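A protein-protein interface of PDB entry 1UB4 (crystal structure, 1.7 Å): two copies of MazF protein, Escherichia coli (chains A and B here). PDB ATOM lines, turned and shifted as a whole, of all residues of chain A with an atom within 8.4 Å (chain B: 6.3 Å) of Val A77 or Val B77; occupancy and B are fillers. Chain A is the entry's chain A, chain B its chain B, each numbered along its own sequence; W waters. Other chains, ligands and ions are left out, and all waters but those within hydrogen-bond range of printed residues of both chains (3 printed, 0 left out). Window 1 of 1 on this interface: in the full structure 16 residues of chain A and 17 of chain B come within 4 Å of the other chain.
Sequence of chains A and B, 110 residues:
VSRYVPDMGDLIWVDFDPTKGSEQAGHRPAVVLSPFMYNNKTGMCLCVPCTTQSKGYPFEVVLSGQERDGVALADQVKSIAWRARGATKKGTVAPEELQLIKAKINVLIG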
ATOM      1  N   VAL A  31      27.852   4.714 -31.434  1.00  0.00           N
ATOM      2  CA  VAL A  31      27.311   3.459 -31.959  1.00  0.00           C
ATOM      3  C   VAL A  31      25.880   3.752 -32.412  1.00  0.00           C
ATOM      4  O   VAL A  31      25.061   4.235 -31.616  1.00  0.00           O
ATOM      5  CB  VAL A  31      27.245   2.364 -30.875  1.00  0.00           C
ATOM      6  CG1 VAL A  31      26.544   1.112 -31.451  1.00  0.00           C
ATOM      7  CG2 VAL A  31      28.643   2.018 -30.394  1.00  0.00           C
ATOM      8  N   LEU A  33      22.073   3.163 -33.284  1.00  0.00           N
ATOM      9  CA  LEU A  33      21.013   2.300 -32.747  1.00  0.00           C
ATOM     10  C   LEU A  33      19.790   2.123 -33.628  1.00  0.00           C
ATOM     11  O   LEU A  33      19.037   1.148 -33.463  1.00  0.00           O
ATOM     12  CB  LEU A  33      20.521   2.837 -31.404  1.00  0.00           C
ATOM     13  CG  LEU A  33      21.525   2.932 -30.273  1.00  0.00           C
ATOM     14  CD1 LEU A  33      20.875   3.665 -29.095  1.00  0.00           C
ATOM     15  CD2 LEU A  33      21.975   1.548 -29.887  1.00  0.00           C
ATOM     16  N   SER A  34      19.577   3.047 -34.553  1.00  0.00           N
ATOM     17  CA  SER A  34      18.402   3.018 -35.428  1.00  0.00           C
ATOM     18  C   SER A  34      18.711   2.415 -36.801  1.00  0.00           C
ATOM     19  O   SER A  34      19.861   2.414 -37.261  1.00  0.00           O
ATOM     20  CB  SER A  34      17.836   4.441 -35.579  1.00  0.00           C
ATOM     21  OG  SER A  34      18.884   5.356 -35.861  1.00  0.00           O
ATOM     22  N   TYR A  38      15.188   4.380 -41.573  1.00  0.00           N
ATOM     23  CA  TYR A  38      14.876   5.587 -40.805  1.00  0.00           C
ATOM     24  C   TYR A  38      16.028   6.580 -40.968  1.00  0.00           C
ATOM     25  O   TYR A  38      15.807   7.764 -41.231  1.00  0.00           O
ATOM     26  CB  TYR A  38      14.721   5.232 -39.314  1.00  0.00           C
ATOM     27  CG  TYR A  38      14.674   6.449 -38.398  1.00  0.00           C
ATOM     28  CD1 TYR A  38      13.467   7.095 -38.114  1.00  0.00           C
ATOM     29  CD2 TYR A  38      15.851   6.990 -37.868  1.00  0.00           C
ATOM     30  CE1 TYR A  38      13.444   8.267 -37.323  1.00  0.00           C
ATOM     31  CE2 TYR A  38      15.839   8.154 -37.082  1.00  0.00           C
ATOM     32  CZ  TYR A  38      14.632   8.783 -36.820  1.00  0.00           C
ATOM     33  OH  TYR A  38      14.637   9.943 -36.072  1.00  0.00           O
ATOM     34  N   CYS A  45      19.638   9.900 -36.674  1.00  0.00           N
ATOM     35  CA  CYS A  45      19.846   8.529 -36.207  1.00  0.00           C
ATOM     36  C   CYS A  45      19.977   8.596 -34.702  1.00  0.00           C
ATOM     37  O   CYS A  45      20.354   9.629 -34.150  1.00  0.00           O
ATOM     38  CB  CYS A  45      21.092   7.877 -36.826  1.00  0.00           C
ATOM     39  SG  CYS A  45      22.689   8.523 -36.319  1.00  0.00           S
ATOM     40  N   LEU A  46      19.596   7.516 -34.039  1.00  0.00           N
ATOM     41  CA  LEU A  46      19.737   7.432 -32.592  1.00  0.00           C
ATOM     42  C   LEU A  46      21.047   6.714 -32.388  1.00  0.00           C
ATOM     43  O   LEU A  46      21.370   5.764 -33.117  1.00  0.00           O
ATOM     44  CB  LEU A  46      18.604   6.606 -31.979  1.00  0.00           C
ATOM     45  CG  LEU A  46      17.286   7.376 -31.828  1.00  0.00           C
ATOM     46  CD1 LEU A  46      16.162   6.395 -31.487  1.00  0.00           C
ATOM     47  CD2 LEU A  46      17.412   8.416 -30.743  1.00  0.00           C
ATOM     48  N   CYS A  47      21.817   7.162 -31.406  1.00  0.00           N
ATOM     49  CA  CYS A  47      23.104   6.531 -31.134  1.00  0.00           C
ATOM     50  C   CYS A  47      23.484   6.727 -29.674  1.00  0.00           C
ATOM     51  O   CYS A  47      22.792   7.428 -28.925  1.00  0.00           O
ATOM     52  CB  CYS A  47      24.197   7.166 -31.991  1.00  0.00           C
ATOM     53  SG  CYS A  47      24.503   8.939 -31.632  1.00  0.00           S
ATOM     54  N   VAL A  48      24.579   6.094 -29.285  1.00  0.00           N
ATOM     55  CA  VAL A  48      25.110   6.267 -27.942  1.00  0.00           C
ATOM     56  C   VAL A  48      26.574   6.598 -28.140  1.00  0.00           C
ATOM     57  O   VAL A  48      27.237   6.051 -29.017  1.00  0.00           O
ATOM     58  CB  VAL A  48      24.959   5.017 -27.052  1.00  0.00           C
ATOM     59  CG1 VAL A  48      23.483   4.862 -26.644  1.00  0.00           C
ATOM     60  CG2 VAL A  48      25.486   3.788 -27.762  1.00  0.00           C
ATOM     61  N   PRO A  49      27.092   7.527 -27.333  1.00  0.00           N
ATOM     62  CA  PRO A  49      28.491   7.935 -27.436  1.00  0.00           C
ATOM     63  C   PRO A  49      29.470   6.935 -26.852  1.00  0.00           C
ATOM     64  O   PRO A  49      29.138   6.176 -25.940  1.00  0.00           O
ATOM     65  CB  PRO A  49      28.519   9.260 -26.676  1.00  0.00           C
ATOM     66  CG  PRO A  49      27.546   8.989 -25.542  1.00  0.00           C
ATOM     67  CD  PRO A  49      26.398   8.236 -26.244  1.00  0.00           C
ATOM     68  N   PHE A  59      26.280   1.463 -16.936  1.00  0.00           N
ATOM     69  CA  PHE A  59      25.729   1.567 -18.288  1.00  0.00           C
ATOM     70  C   PHE A  59      26.804   1.495 -19.369  1.00  0.00           C
ATOM     71  O   PHE A  59      26.514   1.642 -20.559  1.00  0.00           O
ATOM     72  CB  PHE A  59      24.849   2.820 -18.450  1.00  0.00           C
ATOM     73  CG  PHE A  59      23.532   2.707 -17.738  1.00  0.00           C
ATOM     74  CD1 PHE A  59      23.411   3.101 -16.400  1.00  0.00           C
ATOM     75  CD2 PHE A  59      22.442   2.111 -18.365  1.00  0.00           C
ATOM     76  CE1 PHE A  59      22.226   2.898 -15.691  1.00  0.00           C
ATOM     77  CE2 PHE A  59      21.250   1.902 -17.674  1.00  0.00           C
ATOM     78  CZ  PHE A  59      21.137   2.294 -16.333  1.00  0.00           C
ATOM     79  N   LEU A  73      28.455   4.414 -23.800  1.00  0.00           N
ATOM     80  CA  LEU A  73      27.685   4.849 -22.622  1.00  0.00           C
ATOM     81  C   LEU A  73      26.209   4.679 -23.004  1.00  0.00           C
ATOM     82  O   LEU A  73      25.581   5.582 -23.566  1.00  0.00           O
ATOM     83  CB  LEU A  73      28.021   6.299 -22.273  1.00  0.00           C
ATOM     84  CG  LEU A  73      29.498   6.555 -21.954  1.00  0.00           C
ATOM     85  CD1 LEU A  73      29.667   8.040 -21.608  1.00  0.00           C
ATOM     86  CD2 LEU A  73      29.966   5.693 -20.783  1.00  0.00           C
ATOM     87  N   ALA A  74      25.665   3.511 -22.672  1.00  0.00           N
ATOM     88  CA  ALA A  74      24.309   3.166 -23.071  1.00  0.00           C
ATOM     89  C   ALA A  74      23.208   4.095 -22.597  1.00  0.00           C
ATOM     90  O   ALA A  74      22.192   4.226 -23.268  1.00  0.00           O
ATOM     91  CB  ALA A  74      23.984   1.719 -22.649  1.00  0.00           C
ATOM     92  N   ASP A  75      23.386   4.736 -21.446  1.00  0.00           N
ATOM     93  CA  ASP A  75      22.328   5.627 -20.974  1.00  0.00           C
ATOM     94  C   ASP A  75      22.294   7.002 -21.643  1.00  0.00           C
ATOM     95  O   ASP A  75      21.351   7.769 -21.421  1.00  0.00           O
ATOM     96  CB  ASP A  75      22.369   5.769 -19.427  1.00  0.00           C
ATOM     97  CG  ASP A  75      23.674   6.357 -18.904  1.00  0.00           C
ATOM     98  OD1 ASP A  75      23.624   6.942 -17.800  1.00  0.00           O
ATOM     99  OD2 ASP A  75      24.732   6.242 -19.564  1.00  0.00           O
ATOM    100  N   GLN A  76      23.282   7.309 -22.485  1.00  0.00           N
ATOM    101  CA  GLN A  76      23.308   8.605 -23.145  1.00  0.00           C
ATOM    102  C   GLN A  76      22.834   8.563 -24.600  1.00  0.00           C
ATOM    103  O   GLN A  76      23.468   9.126 -25.491  1.00  0.00           O
ATOM    104  CB  GLN A  76      24.704   9.233 -23.032  1.00  0.00           C
ATOM    105  CG  GLN A  76      25.011   9.657 -21.593  1.00  0.00           C
ATOM    106  CD  GLN A  76      26.200  10.599 -21.493  1.00  0.00           C
ATOM    107  OE1 GLN A  76      26.319  11.541 -22.277  1.00  0.00           O
ATOM    108  NE2 GLN A  76      27.071  10.362 -20.515  1.00  0.00           N
ATOM    109  N   VAL A  77      21.707   7.883 -24.798  1.00  0.00           N
ATOM    110  CA  VAL A  77      21.042   7.761 -26.101  1.00  0.00           C
ATOM    111  C   VAL A  77      20.866   9.173 -26.634  1.00  0.00           C
ATOM    112  O   VAL A  77      20.409  10.054 -25.922  1.00  0.00           O
ATOM    113  CB  VAL A  77      19.628   7.137 -25.942  1.00  0.00           C
ATOM    114  CG1 VAL A  77      18.885   7.148 -27.292  1.00  0.00           C
ATOM    115  CG2 VAL A  77      19.744   5.726 -25.405  1.00  0.00           C
ATOM    116  N   LYS A  78      21.192   9.381 -27.906  1.00  0.00           N
ATOM    117  CA  LYS A  78      21.092  10.710 -28.482  1.00  0.00           C
ATOM    118  C   LYS A  78      20.619  10.668 -29.933  1.00  0.00           C
ATOM    119  O   LYS A  78      21.114   9.857 -30.706  1.00  0.00           O
ATOM    120  CB  LYS A  78      22.484  11.360 -28.413  1.00  0.00           C
ATOM    121  CG  LYS A  78      22.655  12.639 -29.199  1.00  0.00           C
ATOM    122  CD  LYS A  78      21.898  13.790 -28.625  1.00  0.00           C
ATOM    123  CE  LYS A  78      22.392  15.091 -29.247  1.00  0.00           C
ATOM    124  NZ  LYS A  78      21.646  16.255 -28.708  1.00  0.00           N
ATOM    125  N   SER A  79      19.659  11.526 -30.281  1.00  0.00           N
ATOM    126  CA  SER A  79      19.186  11.652 -31.665  1.00  0.00           C
ATOM    127  C   SER A  79      20.121  12.695 -32.277  1.00  0.00           C
ATOM    128  O   SER A  79      20.203  13.834 -31.793  1.00  0.00           O
ATOM    129  CB  SER A  79      17.739  12.165 -31.711  1.00  0.00           C
ATOM    130  OG  SER A  79      17.363  12.585 -33.024  1.00  0.00           O
ATOM    131  N   ILE A  80      20.840  12.300 -33.323  1.00  0.00           N
ATOM    132  CA  ILE A  80      21.781  13.207 -33.970  1.00  0.00           C
ATOM    133  C   ILE A  80      21.486  13.401 -35.448  1.00  0.00           C
ATOM    134  O   ILE A  80      21.002  12.489 -36.135  1.00  0.00           O
ATOM    135  CB  ILE A  80      23.232  12.708 -33.848  1.00  0.00           C
ATOM    136  CG1 ILE A  80      23.385  11.344 -34.506  1.00  0.00           C
ATOM    137  CG2 ILE A  80      23.641  12.645 -32.394  1.00  0.00           C
ATOM    138  CD1 ILE A  80      24.835  10.932 -34.688  1.00  0.00           C
ATOM    139  N   ILE A 101      23.997  -3.129 -25.228  1.00  0.00           N
ATOM    140  CA  ILE A 101      23.641  -1.714 -25.206  1.00  0.00           C
ATOM    141  C   ILE A 101      22.131  -1.551 -25.153  1.00  0.00           C
ATOM    142  O   ILE A 101      21.608  -0.797 -24.333  1.00  0.00           O
ATOM    143  CB  ILE A 101      24.203  -0.996 -26.454  1.00  0.00           C
ATOM    144  CG1 ILE A 101      25.721  -0.954 -26.334  1.00  0.00           C
ATOM    145  CG2 ILE A 101      23.615   0.423 -26.609  1.00  0.00           C
ATOM    146  CD1 ILE A 101      26.419  -0.490 -27.599  1.00  0.00           C
ATOM    147  N   LYS A 102      21.440  -2.278 -26.030  1.00  0.00           N
ATOM    148  CA  LYS A 102      19.986  -2.217 -26.124  1.00  0.00           C
ATOM    149  C   LYS A 102      19.288  -2.718 -24.849  1.00  0.00           C
ATOM    150  O   LYS A 102      18.251  -2.183 -24.447  1.00  0.00           O
ATOM    151  CB  LYS A 102      19.497  -3.017 -27.349  1.00  0.00           C
ATOM    152  CG  LYS A 102      19.846  -2.416 -28.754  1.00  0.00           C
ATOM    153  CD  LYS A 102      19.375  -3.371 -29.880  1.00  0.00           C
ATOM    154  CE  LYS A 102      19.780  -2.949 -31.300  1.00  0.00           C
ATOM    155  NZ  LYS A 102      19.455  -4.001 -32.362  1.00  0.00           N
ATOM    156  N   LYS A 104      20.476  -2.528 -21.793  1.00  0.00           N
ATOM    157  CA  LYS A 104      20.676  -1.547 -20.732  1.00  0.00           C
ATOM    158  C   LYS A 104      19.798  -0.329 -20.968  1.00  0.00           C
ATOM    159  O   LYS A 104      19.220   0.231 -20.027  1.00  0.00           O
ATOM    160  CB  LYS A 104      22.175  -1.211 -20.616  1.00  0.00           C
ATOM    161  CG  LYS A 104      22.986  -2.415 -20.074  1.00  0.00           C
ATOM    162  CD  LYS A 104      24.437  -2.063 -19.749  1.00  0.00           C
ATOM    163  CE  LYS A 104      25.140  -3.231 -19.071  1.00  0.00           C
ATOM    164  NZ  LYS A 104      26.556  -2.913 -18.742  1.00  0.00           N
ATOM    165  N   ILE A 105      19.647   0.072 -22.227  1.00  0.00           N
ATOM    166  CA  ILE A 105      18.746   1.180 -22.544  1.00  0.00           C
ATOM    167  C   ILE A 105      17.314   0.800 -22.142  1.00  0.00           C
ATOM    168  O   ILE A 105      16.549   1.629 -21.637  1.00  0.00           O
ATOM    169  CB  ILE A 105      18.732   1.483 -24.067  1.00  0.00           C
ATOM    170  CG1 ILE A 105      20.070   2.074 -24.509  1.00  0.00           C
ATOM    171  CG2 ILE A 105      17.582   2.431 -24.393  1.00  0.00           C
ATOM    172  CD1 ILE A 105      20.240   2.091 -26.036  1.00  0.00           C
ATOM    173  N   ASN A 106      16.948  -0.463 -22.349  1.00  0.00           N
ATOM    174  CA  ASN A 106      15.596  -0.916 -22.049  1.00  0.00           C
ATOM    175  C   ASN A 106      15.169  -0.717 -20.596  1.00  0.00           C
ATOM    176  O   ASN A 106      13.990  -0.548 -20.297  1.00  0.00           O
ATOM    177  CB  ASN A 106      15.456  -2.390 -22.440  1.00  0.00           C
ATOM    178  CG  ASN A 106      14.021  -2.873 -22.359  1.00  0.00           C
ATOM    179  OD1 ASN A 106      13.649  -3.579 -21.421  1.00  0.00           O
ATOM    180  ND2 ASN A 106      13.208  -2.487 -23.332  1.00  0.00           N
ATOM    181  N   LEU A 108      15.875   1.778 -18.810  1.00  0.00           N
ATOM    182  CA  LEU A 108      15.535   3.189 -18.619  1.00  0.00           C
ATOM    183  C   LEU A 108      14.338   3.692 -19.408  1.00  0.00           C
ATOM    184  O   LEU A 108      13.573   4.525 -18.925  1.00  0.00           O
ATOM    185  CB  LEU A 108      16.756   4.068 -18.971  1.00  0.00           C
ATOM    186  CG  LEU A 108      18.005   3.850 -18.101  1.00  0.00           C
ATOM    187  CD1 LEU A 108      19.122   4.815 -18.553  1.00  0.00           C
ATOM    188  CD2 LEU A 108      17.659   4.095 -16.619  1.00  0.00           C
ATOM    189  N   ILE A 109      14.161   3.206 -20.628  1.00  0.00           N
ATOM    190  CA  ILE A 109      13.048   3.726 -21.417  1.00  0.00           C
ATOM    191  C   ILE A 109      12.221   2.649 -22.091  1.00  0.00           C
ATOM    192  O   ILE A 109      11.425   2.936 -22.984  1.00  0.00           O
ATOM    193  CB  ILE A 109      13.566   4.751 -22.470  1.00  0.00           C
ATOM    194  CG1 ILE A 109      14.572   4.094 -23.422  1.00  0.00           C
ATOM    195  CG2 ILE A 109      14.275   5.911 -21.757  1.00  0.00           C
ATOM    196  CD1 ILE A 109      15.007   5.020 -24.569  1.00  0.00           C
ATOM    197  N   LEU B  33      11.464  10.516 -19.777  1.00  0.00           N
ATOM    198  CA  LEU B  33      11.199   9.094 -19.998  1.00  0.00           C
ATOM    199  C   LEU B  33      11.800   8.142 -18.966  1.00  0.00           C
ATOM    200  O   LEU B  33      11.258   7.061 -18.737  1.00  0.00           O
ATOM    201  CB  LEU B  33      11.710   8.670 -21.376  1.00  0.00           C
ATOM    202  CG  LEU B  33      11.132   9.469 -22.555  1.00  0.00           C
ATOM    203  CD1 LEU B  33      11.548   8.810 -23.858  1.00  0.00           C
ATOM    204  CD2 LEU B  33       9.620   9.524 -22.475  1.00  0.00           C
ATOM    205  N   LEU B  46      16.620  10.898 -19.450  1.00  0.00           N
ATOM    206  CA  LEU B  46      16.370  10.710 -20.887  1.00  0.00           C
ATOM    207  C   LEU B  46      14.996  11.338 -21.116  1.00  0.00           C
ATOM    208  O   LEU B  46      14.065  11.148 -20.321  1.00  0.00           O
ATOM    209  CB  LEU B  46      16.365   9.209 -21.259  1.00  0.00           C
ATOM    210  CG  LEU B  46      17.765   8.587 -21.406  1.00  0.00           C
ATOM    211  CD1 LEU B  46      17.692   7.059 -21.474  1.00  0.00           C
ATOM    212  CD2 LEU B  46      18.430   9.145 -22.665  1.00  0.00           C
ATOM    213  N   CYS B  47      14.874  12.098 -22.197  1.00  0.00           N
ATOM    214  CA  CYS B  47      13.625  12.789 -22.501  1.00  0.00           C
ATOM    215  C   CYS B  47      13.455  12.985 -23.998  1.00  0.00           C
ATOM    216  O   CYS B  47      14.368  12.722 -24.774  1.00  0.00           O
ATOM    217  CB  CYS B  47      13.620  14.158 -21.815  1.00  0.00           C
ATOM    218  SG  CYS B  47      15.027  15.221 -22.275  1.00  0.00           S
ATOM    219  N   VAL B  48      12.269  13.428 -24.394  1.00  0.00           N
ATOM    220  CA  VAL B  48      11.996  13.709 -25.797  1.00  0.00           C
ATOM    221  C   VAL B  48      11.441  15.128 -25.820  1.00  0.00           C
ATOM    222  O   VAL B  48      10.702  15.550 -24.927  1.00  0.00           O
ATOM    223  CB  VAL B  48      10.969  12.729 -26.463  1.00  0.00           C
ATOM    224  CG1 VAL B  48      11.634  11.367 -26.693  1.00  0.00           C
ATOM    225  CG2 VAL B  48       9.708  12.608 -25.639  1.00  0.00           C
ATOM    226  N   PRO B  49      11.796  15.894 -26.847  1.00  0.00           N
ATOM    227  CA  PRO B  49      11.313  17.269 -26.948  1.00  0.00           C
ATOM    228  C   PRO B  49       9.838  17.377 -27.338  1.00  0.00           C
ATOM    229  O   PRO B  49       9.276  16.469 -27.965  1.00  0.00           O
ATOM    230  CB  PRO B  49      12.239  17.873 -28.004  1.00  0.00           C
ATOM    231  CG  PRO B  49      12.482  16.707 -28.923  1.00  0.00           C
ATOM    232  CD  PRO B  49      12.647  15.526 -27.997  1.00  0.00           C
ATOM    233  N   LEU B  73       7.943  14.481 -29.684  1.00  0.00           N
ATOM    234  CA  LEU B  73       8.591  13.914 -30.866  1.00  0.00           C
ATOM    235  C   LEU B  73       9.354  12.695 -30.350  1.00  0.00           C
ATOM    236  O   LEU B  73      10.507  12.788 -29.918  1.00  0.00           O
ATOM    237  CB  LEU B  73       9.522  14.957 -31.484  1.00  0.00           C
ATOM    238  CG  LEU B  73       8.769  16.208 -31.957  1.00  0.00           C
ATOM    239  CD1 LEU B  73       9.777  17.242 -32.457  1.00  0.00           C
ATOM    240  CD2 LEU B  73       7.786  15.869 -33.084  1.00  0.00           C
ATOM    241  N   ALA B  74       8.687  11.546 -30.397  1.00  0.00           N
ATOM    242  CA  ALA B  74       9.233  10.308 -29.837  1.00  0.00           C
ATOM    243  C   ALA B  74      10.592   9.815 -30.301  1.00  0.00           C
ATOM    244  O   ALA B  74      11.316   9.219 -29.509  1.00  0.00           O
ATOM    245  CB  ALA B  74       8.190   9.151 -29.979  1.00  0.00           C
ATOM    246  N   ASP B  75      10.949  10.061 -31.557  1.00  0.00           N
ATOM    247  CA  ASP B  75      12.224   9.575 -32.072  1.00  0.00           C
ATOM    248  C   ASP B  75      13.423  10.398 -31.666  1.00  0.00           C
ATOM    249  O   ASP B  75      14.561   9.938 -31.817  1.00  0.00           O
ATOM    250  CB  ASP B  75      12.195   9.466 -33.610  1.00  0.00           C
ATOM    251  CG  ASP B  75      11.894  10.801 -34.312  1.00  0.00           C
ATOM    252  OD1 ASP B  75      12.402  10.990 -35.441  1.00  0.00           O
ATOM    253  OD2 ASP B  75      11.132  11.646 -33.787  1.00  0.00           O
ATOM    254  N   GLN B  76      13.186  11.580 -31.108  1.00  0.00           N
ATOM    255  CA  GLN B  76      14.291  12.456 -30.773  1.00  0.00           C
ATOM    256  C   GLN B  76      14.769  12.473 -29.341  1.00  0.00           C
ATOM    257  O   GLN B  76      14.961  13.520 -28.733  1.00  0.00           O
ATOM    258  CB  GLN B  76      13.954  13.832 -31.287  1.00  0.00           C
ATOM    259  CG  GLN B  76      13.916  13.753 -32.812  1.00  0.00           C
ATOM    260  CD  GLN B  76      13.139  14.859 -33.444  1.00  0.00           C
ATOM    261  OE1 GLN B  76      13.385  16.027 -33.166  1.00  0.00           O
ATOM    262  NE2 GLN B  76      12.184  14.501 -34.316  1.00  0.00           N
ATOM    263  N   VAL B  77      14.996  11.270 -28.845  1.00  0.00           N
ATOM    264  CA  VAL B  77      15.482  11.040 -27.497  1.00  0.00           C
ATOM    265  C   VAL B  77      16.821  11.702 -27.253  1.00  0.00           C
ATOM    266  O   VAL B  77      17.680  11.756 -28.140  1.00  0.00           O
ATOM    267  CB  VAL B  77      15.664   9.530 -27.241  1.00  0.00           C
ATOM    268  CG1 VAL B  77      16.179   9.282 -25.806  1.00  0.00           C
ATOM    269  CG2 VAL B  77      14.355   8.824 -27.468  1.00  0.00           C
ATOM    270  N   LYS B  78      17.001  12.228 -26.047  1.00  0.00           N
ATOM    271  CA  LYS B  78      18.281  12.811 -25.685  1.00  0.00           C
ATOM    272  C   LYS B  78      18.437  12.724 -24.188  1.00  0.00           C
ATOM    273  O   LYS B  78      17.447  12.699 -23.447  1.00  0.00           O
ATOM    274  CB  LYS B  78      18.383  14.273 -26.109  1.00  0.00           C
ATOM    275  CG  LYS B  78      17.367  15.170 -25.446  1.00  0.00           C
ATOM    276  CD  LYS B  78      17.310  16.536 -26.117  1.00  0.00           C
ATOM    277  CE  LYS B  78      16.110  17.330 -25.629  1.00  0.00           C
ATOM    278  NZ  LYS B  78      16.006  18.666 -26.290  1.00  0.00           N
ATOM    279  N   SER B  79      19.689  12.631 -23.758  1.00  0.00           N
ATOM    280  CA  SER B  79      20.007  12.613 -22.343  1.00  0.00           C
ATOM    281  C   SER B  79      20.374  14.042 -21.983  1.00  0.00           C
ATOM    282  O   SER B  79      21.106  14.708 -22.720  1.00  0.00           O
ATOM    283  CB  SER B  79      21.214  11.723 -22.044  1.00  0.00           C
ATOM    284  OG  SER B  79      21.611  11.898 -20.691  1.00  0.00           O
ATOM    285  N   ILE B 105       9.684   4.262 -29.805  1.00  0.00           N
ATOM    286  CA  ILE B 105      11.132   4.164 -29.658  1.00  0.00           C
ATOM    287  C   ILE B 105      11.581   2.713 -29.761  1.00  0.00           C
ATOM    288  O   ILE B 105      12.595   2.418 -30.401  1.00  0.00           O
ATOM    289  CB  ILE B 105      11.598   4.765 -28.297  1.00  0.00           C
ATOM    290  CG1 ILE B 105      11.336   6.276 -28.317  1.00  0.00           C
ATOM    291  CG2 ILE B 105      13.078   4.448 -28.045  1.00  0.00           C
ATOM    292  CD1 ILE B 105      11.416   6.950 -26.983  1.00  0.00           C
ATOM    293  N   ILE B 109      14.497   1.277 -32.242  1.00  0.00           N
ATOM    294  CA  ILE B 109      15.774   0.699 -31.839  1.00  0.00           C
ATOM    295  C   ILE B 109      15.723  -0.711 -31.259  1.00  0.00           C
ATOM    296  O   ILE B 109      16.449  -1.603 -31.722  1.00  0.00           O
ATOM    297  CB  ILE B 109      16.526   1.644 -30.855  1.00  0.00           C
ATOM    298  CG1 ILE B 109      15.685   1.931 -29.614  1.00  0.00           C
ATOM    299  CG2 ILE B 109      16.837   2.970 -31.553  1.00  0.00           C
ATOM    300  CD1 ILE B 109      16.359   2.885 -28.633  1.00  0.00           C
HETATM  301  O   HOH W   1      20.614   9.704 -19.573  1.00  0.00           O
HETATM  302  O   HOH W   2      16.313  10.190 -33.831  1.00  0.00           O
HETATM  303  O   HOH W   3      21.960  12.339 -25.343  1.00  0.00           O
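O of Leu A108 lies close to O of Leu B33. The backbone carbonyl oxygen (O) of Val B77 sits at hydrogen-bond distance from the backbone NH (N) of Ser A79 (2.9 Å). OH of Tyr A38 sits at hydrogen-bond distance from OD1 of Asp B75 (2.5 Å). N of Ser B79 sits at hydrogen-bond distance from O of Val A77.
The backbone carbonyl oxygen of Cys A47 is in hydrogen-bond range of the backbone NH of Lys A78 (2.7 Å). The backbone carbonyl oxygen of Leu B46 sits at hydrogen-bond distance from the backbone NH of Leu B33 (2.7 Å). OD2 of Asp B75 is in hydrogen-bond range of NE2 of Gln B76 (3.1 Å). The backbone carbonyl oxygen of Lys B78 sits at hydrogen-bond distance from the backbone NH of Cys B47 (2.9 Å). OG of Ser A34 sits at hydrogen-bond distance from N of Leu A46, 2.9 Å away. The backbone carbonyl oxygen of Leu A46 sits at hydrogen-bond distance from the backbone NH of Leu A33 (2.7 Å).
Among the printed residues, merely in contact across the chains: Leu A33 with Ile B109, Leu A46 with Asp B75, Leu A46 with Ile B109, Asp A75 with Leu B46, Gln A76 with Ser B79, Val A77 with Leu B46, Val A77 with Val B77, Val A77 with Lys B78, Lys A78 with Val B77, Ser A79 with Asp B75, Ser A79 with Gln B76, Lys A102 with Ile B109, Leu A108 with Leu B46, Ile A109 with Leu B33 and Ile A109 with Leu B46.
Val A48 touches none of the printed residues of chain B. Val A77 touches just these residues of chain B: Leu B46, Val B77, Lys B78 and Ser B79. Printed residues of chain B within 4 Å of Ser A79: Asp B75, Gln B76 and Val B77. Ile A80 touches none of the printed residues of chain B. Of the printed residues of chain B, Ile A109 touches Leu B33 (3.8 Å) and Leu B46 (3.6 Å). Of chain A, only Val A77 (3.8 Å), Lys A78 (3.6 Å) and Ser A79 (2.9 Å) come within 4 Å of Val B77. Of the printed residues of chain A, Lys B78 touches Val A77. The nearest residue of chain B that does not touch Val A77 is Ile B109 (5.1 Å). The nearest printed residue of chain A that does not touch Lys B78 is Lys A78 (4.3 Å).
Of the 14 printed residues of chain B, 8 touch a printed residue of chain A. Printed residues of chain B that touch a printed residue of chain A: Leu B33, Leu B46, Asp B75, Gln B76, Val B77, Lys B78, Ser B79 and Ile B109. Of the 25 printed residues of chain A, 11 touch a printed residue of chain B. Hydrophobic or aromatic side chains of chain A within 4 Å of the printed part of chain B: Leu A33, Tyr A38, Leu A46, Val A77, Leu A108 and Ile A109.
Leu A33 touches Ile B109, and with the chains exchanged Ile A109 touches Leu B33. Leu A46 touches Ile B109, and with the chains exchanged Ile A109 touches Leu B46. Gln A76 touches Ser B79, and with the chains exchanged Ser A79 touches Gln B76. Ser A79 touches Asp B75, but with the chains exchanged Asp A75 does not touch Ser B79 (4.01 Å).
Water W1 lies within hydrogen-bond range of the side-chain hydroxyl (OG) of Ser B79 and the backbone carbonyl oxygen (O) of Asp A75. Water W2 lies within hydrogen-bond range of O of Asp B75 (2.7 Å), OG of Ser A79 (2.7 Å) and OH of Tyr A38 (2.8 Å). Water W3 lies within hydrogen-bond range of the backbone NH (N) of Ser B79 (2.8 Å) and the backbone carbonyl oxygen (O) of Val A77 (2.8 Å).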
